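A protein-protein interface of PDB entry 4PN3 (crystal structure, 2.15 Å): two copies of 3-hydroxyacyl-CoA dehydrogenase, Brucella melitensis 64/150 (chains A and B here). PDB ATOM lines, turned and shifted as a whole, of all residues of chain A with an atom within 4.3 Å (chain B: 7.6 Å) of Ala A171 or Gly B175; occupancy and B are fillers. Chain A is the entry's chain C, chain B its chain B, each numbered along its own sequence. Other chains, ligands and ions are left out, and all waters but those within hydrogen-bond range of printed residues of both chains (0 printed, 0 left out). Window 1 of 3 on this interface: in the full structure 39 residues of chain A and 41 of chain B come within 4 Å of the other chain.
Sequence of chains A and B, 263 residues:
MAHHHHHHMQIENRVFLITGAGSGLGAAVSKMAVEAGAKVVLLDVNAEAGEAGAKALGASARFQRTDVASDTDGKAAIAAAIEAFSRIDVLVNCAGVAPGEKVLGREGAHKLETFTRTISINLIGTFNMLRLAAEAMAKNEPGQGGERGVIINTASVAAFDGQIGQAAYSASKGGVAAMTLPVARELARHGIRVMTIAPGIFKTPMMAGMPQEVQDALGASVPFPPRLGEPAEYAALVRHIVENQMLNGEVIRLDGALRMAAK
Among the printed residues, pairs that only touch across the chains: Phe A115 with Phe B127 (3.2 Å), Ala A167 with Phe B127 (3.9 Å), Ala A167 with Met B179 (3.7 Å), Ser A170 with Ala B178 (3.7 Å), Ser A170 with Pro B182 (3.6 Å), Ala A171 with Gly B175 (3.4 Å), Ala A171 with Met B179 (3.6 Å), Gly A174 with Ala B178 (3.8 Å) and Gly A175 with Ala B171 (3.3 Å).
Ala A171 touches just these residues of chain B: Gly B175 (3.4 Å) and Met B179 (3.6 Å).
Printed residues of chain B within 4 Å of Ser A170: Ala B178 (3.7 Å) and Pro B182 (3.6 Å).
Printed residues of chain B within 4 Å of Phe A115: Phe B127 (3.2 Å).
Of the printed residues of chain A, Pro B182 touches Ser A170.
The nearest printed residue of chain A that does not touch Gly B175 is Gly A175 (4.02 Å).
The nearest printed residue of chain B that does not touch Gly A174 is Gly B174 (4.1 Å).
Printed residues of chain A that touch a printed residue of chain B: Phe A115, Ala A167, Ser A170, Ala A171, Gly A174 and Gly A175.
Hydrophobic or aromatic side chains of chain A that line the printed part of chain B: Phe A115, Ala A167 and Ala A171.
Of the 20 printed residues of chain B, 6 touch a printed residue of chain A.
Hydrophobic or aromatic side chains of chain B within 4 Å of the printed part of chain A: Phe B127, Ala B171, Ala B178, Met B179 and Pro B182.
Among the printed residues, no Asp or Glu carboxylate lies within 4 Å of a Lys or Arg side-chain nitrogen of the other chain.
Ala A171 touches Gly B175, and with the chains exchanged Gly A175 touches Ala B171.
Positions printed for both chains: 169, 170, 171, 172, 173, 174 and 175.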
ATOM      1  N   PHE A 115     -17.704  -4.389  10.541  1.00  0.00           N
ATOM      2  CA  PHE A 115     -16.817  -4.901   9.542  1.00  0.00           C
ATOM      3  C   PHE A 115     -16.938  -6.431   9.443  1.00  0.00           C
ATOM      4  O   PHE A 115     -17.119  -6.994   8.352  1.00  0.00           O
ATOM      5  CB  PHE A 115     -15.386  -4.527   9.896  1.00  0.00           C
ATOM      6  CG  PHE A 115     -14.399  -4.849   8.829  1.00  0.00           C
ATOM      7  CD1 PHE A 115     -13.850  -6.110   8.749  1.00  0.00           C
ATOM      8  CD2 PHE A 115     -14.004  -3.883   7.901  1.00  0.00           C
ATOM      9  CE1 PHE A 115     -12.923  -6.406   7.766  1.00  0.00           C
ATOM     10  CE2 PHE A 115     -13.100  -4.189   6.895  1.00  0.00           C
ATOM     11  CZ  PHE A 115     -12.548  -5.450   6.853  1.00  0.00           C
ATOM     12  N   ALA A 167     -14.889   0.530   3.103  1.00  0.00           N
ATOM     13  CA  ALA A 167     -13.788  -0.382   3.428  1.00  0.00           C
ATOM     14  C   ALA A 167     -14.311  -1.810   3.578  1.00  0.00           C
ATOM     15  O   ALA A 167     -13.792  -2.747   2.955  1.00  0.00           O
ATOM     16  CB  ALA A 167     -13.080   0.053   4.689  1.00  0.00           C
ATOM     17  N   ALA A 168     -15.363  -1.985   4.389  1.00  0.00           N
ATOM     18  CA  ALA A 168     -15.898  -3.312   4.637  1.00  0.00           C
ATOM     19  C   ALA A 168     -16.416  -3.943   3.362  1.00  0.00           C
ATOM     20  O   ALA A 168     -16.085  -5.080   3.059  1.00  0.00           O
ATOM     21  CB  ALA A 168     -17.011  -3.269   5.690  1.00  0.00           C
ATOM     22  N   TYR A 169     -17.261  -3.213   2.656  1.00  0.00           N
ATOM     23  CA  TYR A 169     -17.907  -3.696   1.441  1.00  0.00           C
ATOM     24  C   TYR A 169     -16.846  -4.051   0.396  1.00  0.00           C
ATOM     25  O   TYR A 169     -16.931  -5.098  -0.226  1.00  0.00           O
ATOM     26  CB  TYR A 169     -18.896  -2.638   0.890  1.00  0.00           C
ATOM     27  CG  TYR A 169     -19.801  -3.150  -0.214  1.00  0.00           C
ATOM     28  CD1 TYR A 169     -20.564  -4.276  -0.035  1.00  0.00           C
ATOM     29  CD2 TYR A 169     -19.898  -2.480  -1.434  1.00  0.00           C
ATOM     30  CE1 TYR A 169     -21.387  -4.758  -1.040  1.00  0.00           C
ATOM     31  CE2 TYR A 169     -20.723  -2.947  -2.451  1.00  0.00           C
ATOM     32  CZ  TYR A 169     -21.462  -4.093  -2.247  1.00  0.00           C
ATOM     33  OH  TYR A 169     -22.289  -4.581  -3.246  1.00  0.00           O
ATOM     34  N   SER A 170     -15.884  -3.140   0.192  1.00  0.00           N
ATOM     35  CA  SER A 170     -14.806  -3.382  -0.796  1.00  0.00           C
ATOM     36  C   SER A 170     -13.983  -4.568  -0.421  1.00  0.00           C
ATOM     37  O   SER A 170     -13.665  -5.390  -1.267  1.00  0.00           O
ATOM     38  CB  SER A 170     -13.891  -2.176  -0.950  1.00  0.00           C
ATOM     39  OG  SER A 170     -14.601  -1.084  -1.503  1.00  0.00           O
ATOM     40  N   ALA A 171     -13.646  -4.679   0.857  1.00  0.00           N
ATOM     41  CA  ALA A 171     -12.901  -5.846   1.340  1.00  0.00           C
ATOM     42  C   ALA A 171     -13.634  -7.154   1.056  1.00  0.00           C
ATOM     43  O   ALA A 171     -13.035  -8.122   0.584  1.00  0.00           O
ATOM     44  CB  ALA A 171     -12.609  -5.713   2.843  1.00  0.00           C
ATOM     45  N   SER A 172     -14.925  -7.203   1.386  1.00  0.00           N
ATOM     46  CA  SER A 172     -15.650  -8.431   1.196  1.00  0.00           C
ATOM     47  C   SER A 172     -15.788  -8.786  -0.305  1.00  0.00           C
ATOM     48  O   SER A 172     -15.572  -9.917  -0.703  1.00  0.00           O
ATOM     49  CB  SER A 172     -17.030  -8.365   1.890  1.00  0.00           C
ATOM     50  OG  SER A 172     -17.880  -7.408   1.286  1.00  0.00           O
ATOM     51  N   LYS A 173     -16.114  -7.805  -1.131  1.00  0.00           N
ATOM     52  CA  LYS A 173     -16.297  -8.058  -2.561  1.00  0.00           C
ATOM     53  C   LYS A 173     -14.979  -8.239  -3.310  1.00  0.00           C
ATOM     54  O   LYS A 173     -14.918  -8.993  -4.294  1.00  0.00           O
ATOM     55  CB  LYS A 173     -17.114  -6.939  -3.181  1.00  0.00           C
ATOM     56  CG  LYS A 173     -18.506  -6.792  -2.587  1.00  0.00           C
ATOM     57  CD  LYS A 173     -19.231  -8.120  -2.553  1.00  0.00           C
ATOM     58  CE  LYS A 173     -20.710  -7.912  -2.396  1.00  0.00           C
ATOM     59  NZ  LYS A 173     -21.467  -9.043  -2.992  1.00  0.00           N
ATOM     60  N   GLY A 174     -13.927  -7.567  -2.867  1.00  0.00           N
ATOM     61  CA  GLY A 174     -12.607  -7.827  -3.427  1.00  0.00           C
ATOM     62  C   GLY A 174     -12.180  -9.271  -3.132  1.00  0.00           C
ATOM     63  O   GLY A 174     -11.475  -9.912  -3.946  1.00  0.00           O
ATOM     64  N   GLY A 175     -12.589  -9.764  -1.959  1.00  0.00           N
ATOM     65  CA  GLY A 175     -12.280 -11.119  -1.550  1.00  0.00           C
ATOM     66  C   GLY A 175     -12.972 -12.123  -2.406  1.00  0.00           C
ATOM     67  O   GLY A 175     -12.363 -13.107  -2.851  1.00  0.00           O
ATOM     68  N   ASN B 122      -5.706 -12.413   8.676  1.00  0.00           N
ATOM     69  CA  ASN B 122      -5.153 -11.650   7.547  1.00  0.00           C
ATOM     70  C   ASN B 122      -5.897 -10.360   7.212  1.00  0.00           C
ATOM     71  O   ASN B 122      -5.276  -9.318   6.981  1.00  0.00           O
ATOM     72  CB  ASN B 122      -5.144 -12.517   6.297  1.00  0.00           C
ATOM     73  CG  ASN B 122      -4.168 -13.684   6.390  1.00  0.00           C
ATOM     74  OD1 ASN B 122      -3.374 -13.793   7.329  1.00  0.00           O
ATOM     75  ND2 ASN B 122      -4.140 -14.507   5.345  1.00  0.00           N
ATOM     76  N   LEU B 123      -7.219 -10.419   7.206  1.00  0.00           N
ATOM     77  CA  LEU B 123      -8.028  -9.294   6.780  1.00  0.00           C
ATOM     78  C   LEU B 123      -8.656  -8.508   7.940  1.00  0.00           C
ATOM     79  O   LEU B 123      -8.513  -7.285   8.032  1.00  0.00           O
ATOM     80  CB  LEU B 123      -9.123  -9.792   5.826  1.00  0.00           C
ATOM     81  CG  LEU B 123     -10.142  -8.794   5.268  1.00  0.00           C
ATOM     82  CD1 LEU B 123      -9.453  -7.633   4.559  1.00  0.00           C
ATOM     83  CD2 LEU B 123     -11.126  -9.494   4.339  1.00  0.00           C
ATOM     84  N   THR B 126      -5.868  -6.932   9.965  1.00  0.00           N
ATOM     85  CA  THR B 126      -5.321  -5.781   9.282  1.00  0.00           C
ATOM     86  C   THR B 126      -6.232  -4.575   9.409  1.00  0.00           C
ATOM     87  O   THR B 126      -5.783  -3.472   9.735  1.00  0.00           O
ATOM     88  CB  THR B 126      -5.005  -6.145   7.807  1.00  0.00           C
ATOM     89  OG1 THR B 126      -3.758  -6.851   7.799  1.00  0.00           O
ATOM     90  CG2 THR B 126      -4.900  -4.940   6.926  1.00  0.00           C
ATOM     91  N   PHE B 127      -7.516  -4.776   9.177  1.00  0.00           N
ATOM     92  CA  PHE B 127      -8.472  -3.663   9.288  1.00  0.00           C
ATOM     93  C   PHE B 127      -8.478  -3.126  10.707  1.00  0.00           C
ATOM     94  O   PHE B 127      -8.522  -1.921  10.905  1.00  0.00           O
ATOM     95  CB  PHE B 127      -9.908  -4.057   8.883  1.00  0.00           C
ATOM     96  CG  PHE B 127     -10.895  -2.913   8.982  1.00  0.00           C
ATOM     97  CD1 PHE B 127     -10.816  -1.856   8.118  1.00  0.00           C
ATOM     98  CD2 PHE B 127     -11.846  -2.879   9.986  1.00  0.00           C
ATOM     99  CE1 PHE B 127     -11.625  -0.762   8.239  1.00  0.00           C
ATOM    100  CE2 PHE B 127     -12.724  -1.824  10.067  1.00  0.00           C
ATOM    101  CZ  PHE B 127     -12.602  -0.753   9.189  1.00  0.00           C
ATOM    102  N   ALA B 155      -0.441  -7.675   1.255  1.00  0.00           N
ATOM    103  CA  ALA B 155      -1.297  -8.589   0.588  1.00  0.00           C
ATOM    104  C   ALA B 155      -0.441  -9.764   0.145  1.00  0.00           C
ATOM    105  O   ALA B 155       0.267 -10.345   0.986  1.00  0.00           O
ATOM    106  CB  ALA B 155      -2.007  -7.898  -0.595  1.00  0.00           C
ATOM    107  N   ALA B 159      -3.359 -12.679  -4.285  1.00  0.00           N
ATOM    108  CA  ALA B 159      -4.478 -11.784  -4.631  1.00  0.00           C
ATOM    109  C   ALA B 159      -4.716 -11.696  -6.130  1.00  0.00           C
ATOM    110  O   ALA B 159      -5.775 -11.278  -6.563  1.00  0.00           O
ATOM    111  CB  ALA B 159      -4.252 -10.386  -4.061  1.00  0.00           C
ATOM    112  N   TYR B 169      -6.632 -17.916   1.501  1.00  0.00           N
ATOM    113  CA  TYR B 169      -5.522 -16.991   1.419  1.00  0.00           C
ATOM    114  C   TYR B 169      -5.788 -15.913   0.378  1.00  0.00           C
ATOM    115  O   TYR B 169      -5.582 -14.728   0.657  1.00  0.00           O
ATOM    116  CB  TYR B 169      -4.201 -17.738   1.093  1.00  0.00           C
ATOM    117  CG  TYR B 169      -2.948 -16.903   1.293  1.00  0.00           C
ATOM    118  CD1 TYR B 169      -2.711 -16.256   2.496  1.00  0.00           C
ATOM    119  CD2 TYR B 169      -1.990 -16.767   0.288  1.00  0.00           C
ATOM    120  CE1 TYR B 169      -1.576 -15.478   2.684  1.00  0.00           C
ATOM    121  CE2 TYR B 169      -0.837 -16.009   0.476  1.00  0.00           C
ATOM    122  CZ  TYR B 169      -0.645 -15.364   1.677  1.00  0.00           C
ATOM    123  OH  TYR B 169       0.472 -14.591   1.892  1.00  0.00           O
ATOM    124  N   SER B 170      -6.234 -16.310  -0.820  1.00  0.00           N
ATOM    125  CA  SER B 170      -6.505 -15.331  -1.895  1.00  0.00           C
ATOM    126  C   SER B 170      -7.619 -14.402  -1.524  1.00  0.00           C
ATOM    127  O   SER B 170      -7.525 -13.212  -1.753  1.00  0.00           O
ATOM    128  CB  SER B 170      -6.843 -16.014  -3.211  1.00  0.00           C
ATOM    129  OG  SER B 170      -5.719 -16.731  -3.710  1.00  0.00           O
ATOM    130  N   ALA B 171      -8.679 -14.953  -0.922  1.00  0.00           N
ATOM    131  CA  ALA B 171      -9.804 -14.156  -0.445  1.00  0.00           C
ATOM    132  C   ALA B 171      -9.387 -13.113   0.580  1.00  0.00           C
ATOM    133  O   ALA B 171      -9.720 -11.926   0.453  1.00  0.00           O
ATOM    134  CB  ALA B 171     -10.884 -15.048   0.153  1.00  0.00           C
ATOM    135  N   SER B 172      -8.629 -13.531   1.586  1.00  0.00           N
ATOM    136  CA  SER B 172      -8.179 -12.591   2.594  1.00  0.00           C
ATOM    137  C   SER B 172      -7.245 -11.497   1.968  1.00  0.00           C
ATOM    138  O   SER B 172      -7.390 -10.303   2.244  1.00  0.00           O
ATOM    139  CB  SER B 172      -7.500 -13.309   3.728  1.00  0.00           C
ATOM    140  OG  SER B 172      -6.264 -13.912   3.375  1.00  0.00           O
ATOM    141  N   LYS B 173      -6.287 -11.905   1.157  1.00  0.00           N
ATOM    142  CA  LYS B 173      -5.322 -10.928   0.591  1.00  0.00           C
ATOM    143  C   LYS B 173      -5.918 -10.062  -0.517  1.00  0.00           C
ATOM    144  O   LYS B 173      -5.531  -8.907  -0.686  1.00  0.00           O
ATOM    145  CB  LYS B 173      -4.065 -11.644   0.098  1.00  0.00           C
ATOM    146  CG  LYS B 173      -3.331 -12.398   1.178  1.00  0.00           C
ATOM    147  CD  LYS B 173      -3.070 -11.500   2.402  1.00  0.00           C
ATOM    148  CE  LYS B 173      -1.984 -12.077   3.264  1.00  0.00           C
ATOM    149  NZ  LYS B 173      -1.293 -11.014   4.029  1.00  0.00           N
ATOM    150  N   GLY B 174      -6.848 -10.605  -1.280  1.00  0.00           N
ATOM    151  CA  GLY B 174      -7.590  -9.803  -2.252  1.00  0.00           C
ATOM    152  C   GLY B 174      -8.391  -8.731  -1.550  1.00  0.00           C
ATOM    153  O   GLY B 174      -8.569  -7.616  -2.061  1.00  0.00           O
ATOM    154  N   GLY B 175      -8.952  -9.098  -0.394  1.00  0.00           N
ATOM    155  CA  GLY B 175      -9.683  -8.157   0.442  1.00  0.00           C
ATOM    156  C   GLY B 175      -8.824  -7.011   0.945  1.00  0.00           C
ATOM    157  O   GLY B 175      -9.249  -5.854   0.898  1.00  0.00           O
ATOM    158  N   VAL B 176      -7.640  -7.341   1.446  1.00  0.00           N
ATOM    159  CA  VAL B 176      -6.657  -6.321   1.824  1.00  0.00           C
ATOM    160  C   VAL B 176      -6.344  -5.392   0.649  1.00  0.00           C
ATOM    161  O   VAL B 176      -6.475  -4.180   0.759  1.00  0.00           O
ATOM    162  CB  VAL B 176      -5.352  -6.944   2.336  1.00  0.00           C
ATOM    163  CG1 VAL B 176      -4.292  -5.887   2.500  1.00  0.00           C
ATOM    164  CG2 VAL B 176      -5.576  -7.661   3.669  1.00  0.00           C
ATOM    165  N   ALA B 177      -5.972  -5.961  -0.481  1.00  0.00           N
ATOM    166  CA  ALA B 177      -5.697  -5.157  -1.679  1.00  0.00           C
ATOM    167  C   ALA B 177      -6.845  -4.205  -2.073  1.00  0.00           C
ATOM    168  O   ALA B 177      -6.611  -3.025  -2.352  1.00  0.00           O
ATOM    169  CB  ALA B 177      -5.354  -6.051  -2.863  1.00  0.00           C
ATOM    170  N   ALA B 178      -8.080  -4.695  -2.044  1.00  0.00           N
ATOM    171  CA  ALA B 178      -9.209  -3.912  -2.506  1.00  0.00           C
ATOM    172  C   ALA B 178      -9.638  -2.778  -1.543  1.00  0.00           C
ATOM    173  O   ALA B 178     -10.271  -1.840  -1.970  1.00  0.00           O
ATOM    174  CB  ALA B 178     -10.375  -4.826  -2.785  1.00  0.00           C
ATOM    175  N   MET B 179      -9.261  -2.868  -0.266  1.00  0.00           N
ATOM    176  CA  MET B 179      -9.521  -1.817   0.711  1.00  0.00           C
ATOM    177  C   MET B 179      -8.665  -0.620   0.555  1.00  0.00           C
ATOM    178  O   MET B 179      -8.967   0.453   1.087  1.00  0.00           O
ATOM    179  CB  MET B 179      -9.148  -2.287   2.112  1.00  0.00           C
ATOM    180  CG  MET B 179     -10.130  -3.141   2.794  1.00  0.00           C
ATOM    181  SD  MET B 179      -9.753  -3.205   4.553  1.00  0.00           S
ATOM    182  CE  MET B 179      -8.098  -3.780   4.736  1.00  0.00           C
ATOM    183  N   THR B 180      -7.529  -0.801  -0.098  1.00  0.00           N
ATOM    184  CA  THR B 180      -6.532   0.256  -0.137  1.00  0.00           C
ATOM    185  C   THR B 180      -7.142   1.555  -0.574  1.00  0.00           C
ATOM    186  O   THR B 180      -6.898   2.610   0.026  1.00  0.00           O
ATOM    187  CB  THR B 180      -5.372  -0.121  -1.061  1.00  0.00           C
ATOM    188  OG1 THR B 180      -4.947  -1.465  -0.781  1.00  0.00           O
ATOM    189  CG2 THR B 180      -4.185   0.808  -0.845  1.00  0.00           C
ATOM    190  N   PRO B 182     -10.541   2.738  -1.084  1.00  0.00           N
ATOM    191  CA  PRO B 182     -11.535   3.443  -0.276  1.00  0.00           C
ATOM    192  C   PRO B 182     -10.977   4.026   1.024  1.00  0.00           C
ATOM    193  O   PRO B 182     -11.480   5.044   1.516  1.00  0.00           O
ATOM    194  CB  PRO B 182     -12.620   2.361   0.009  1.00  0.00           C
ATOM    195  CG  PRO B 182     -11.970   1.072  -0.273  1.00  0.00           C
ATOM    196  CD  PRO B 182     -10.942   1.361  -1.367  1.00  0.00           C
ATOM    197  N   THR B 196      -0.271  -0.629  -0.145  1.00  0.00           N
ATOM    198  CA  THR B 196      -0.269  -2.093   0.017  1.00  0.00           C
ATOM    199  C   THR B 196       0.881  -2.693  -0.804  1.00  0.00           C
ATOM    200  O   THR B 196       1.103  -2.285  -1.962  1.00  0.00           O
ATOM    201  CB  THR B 196      -1.581  -2.680  -0.447  1.00  0.00           C
ATOM    202  OG1 THR B 196      -2.654  -2.281   0.448  1.00  0.00           O
ATOM    203  CG2 THR B 196      -1.474  -4.202  -0.447  1.00  0.00           C
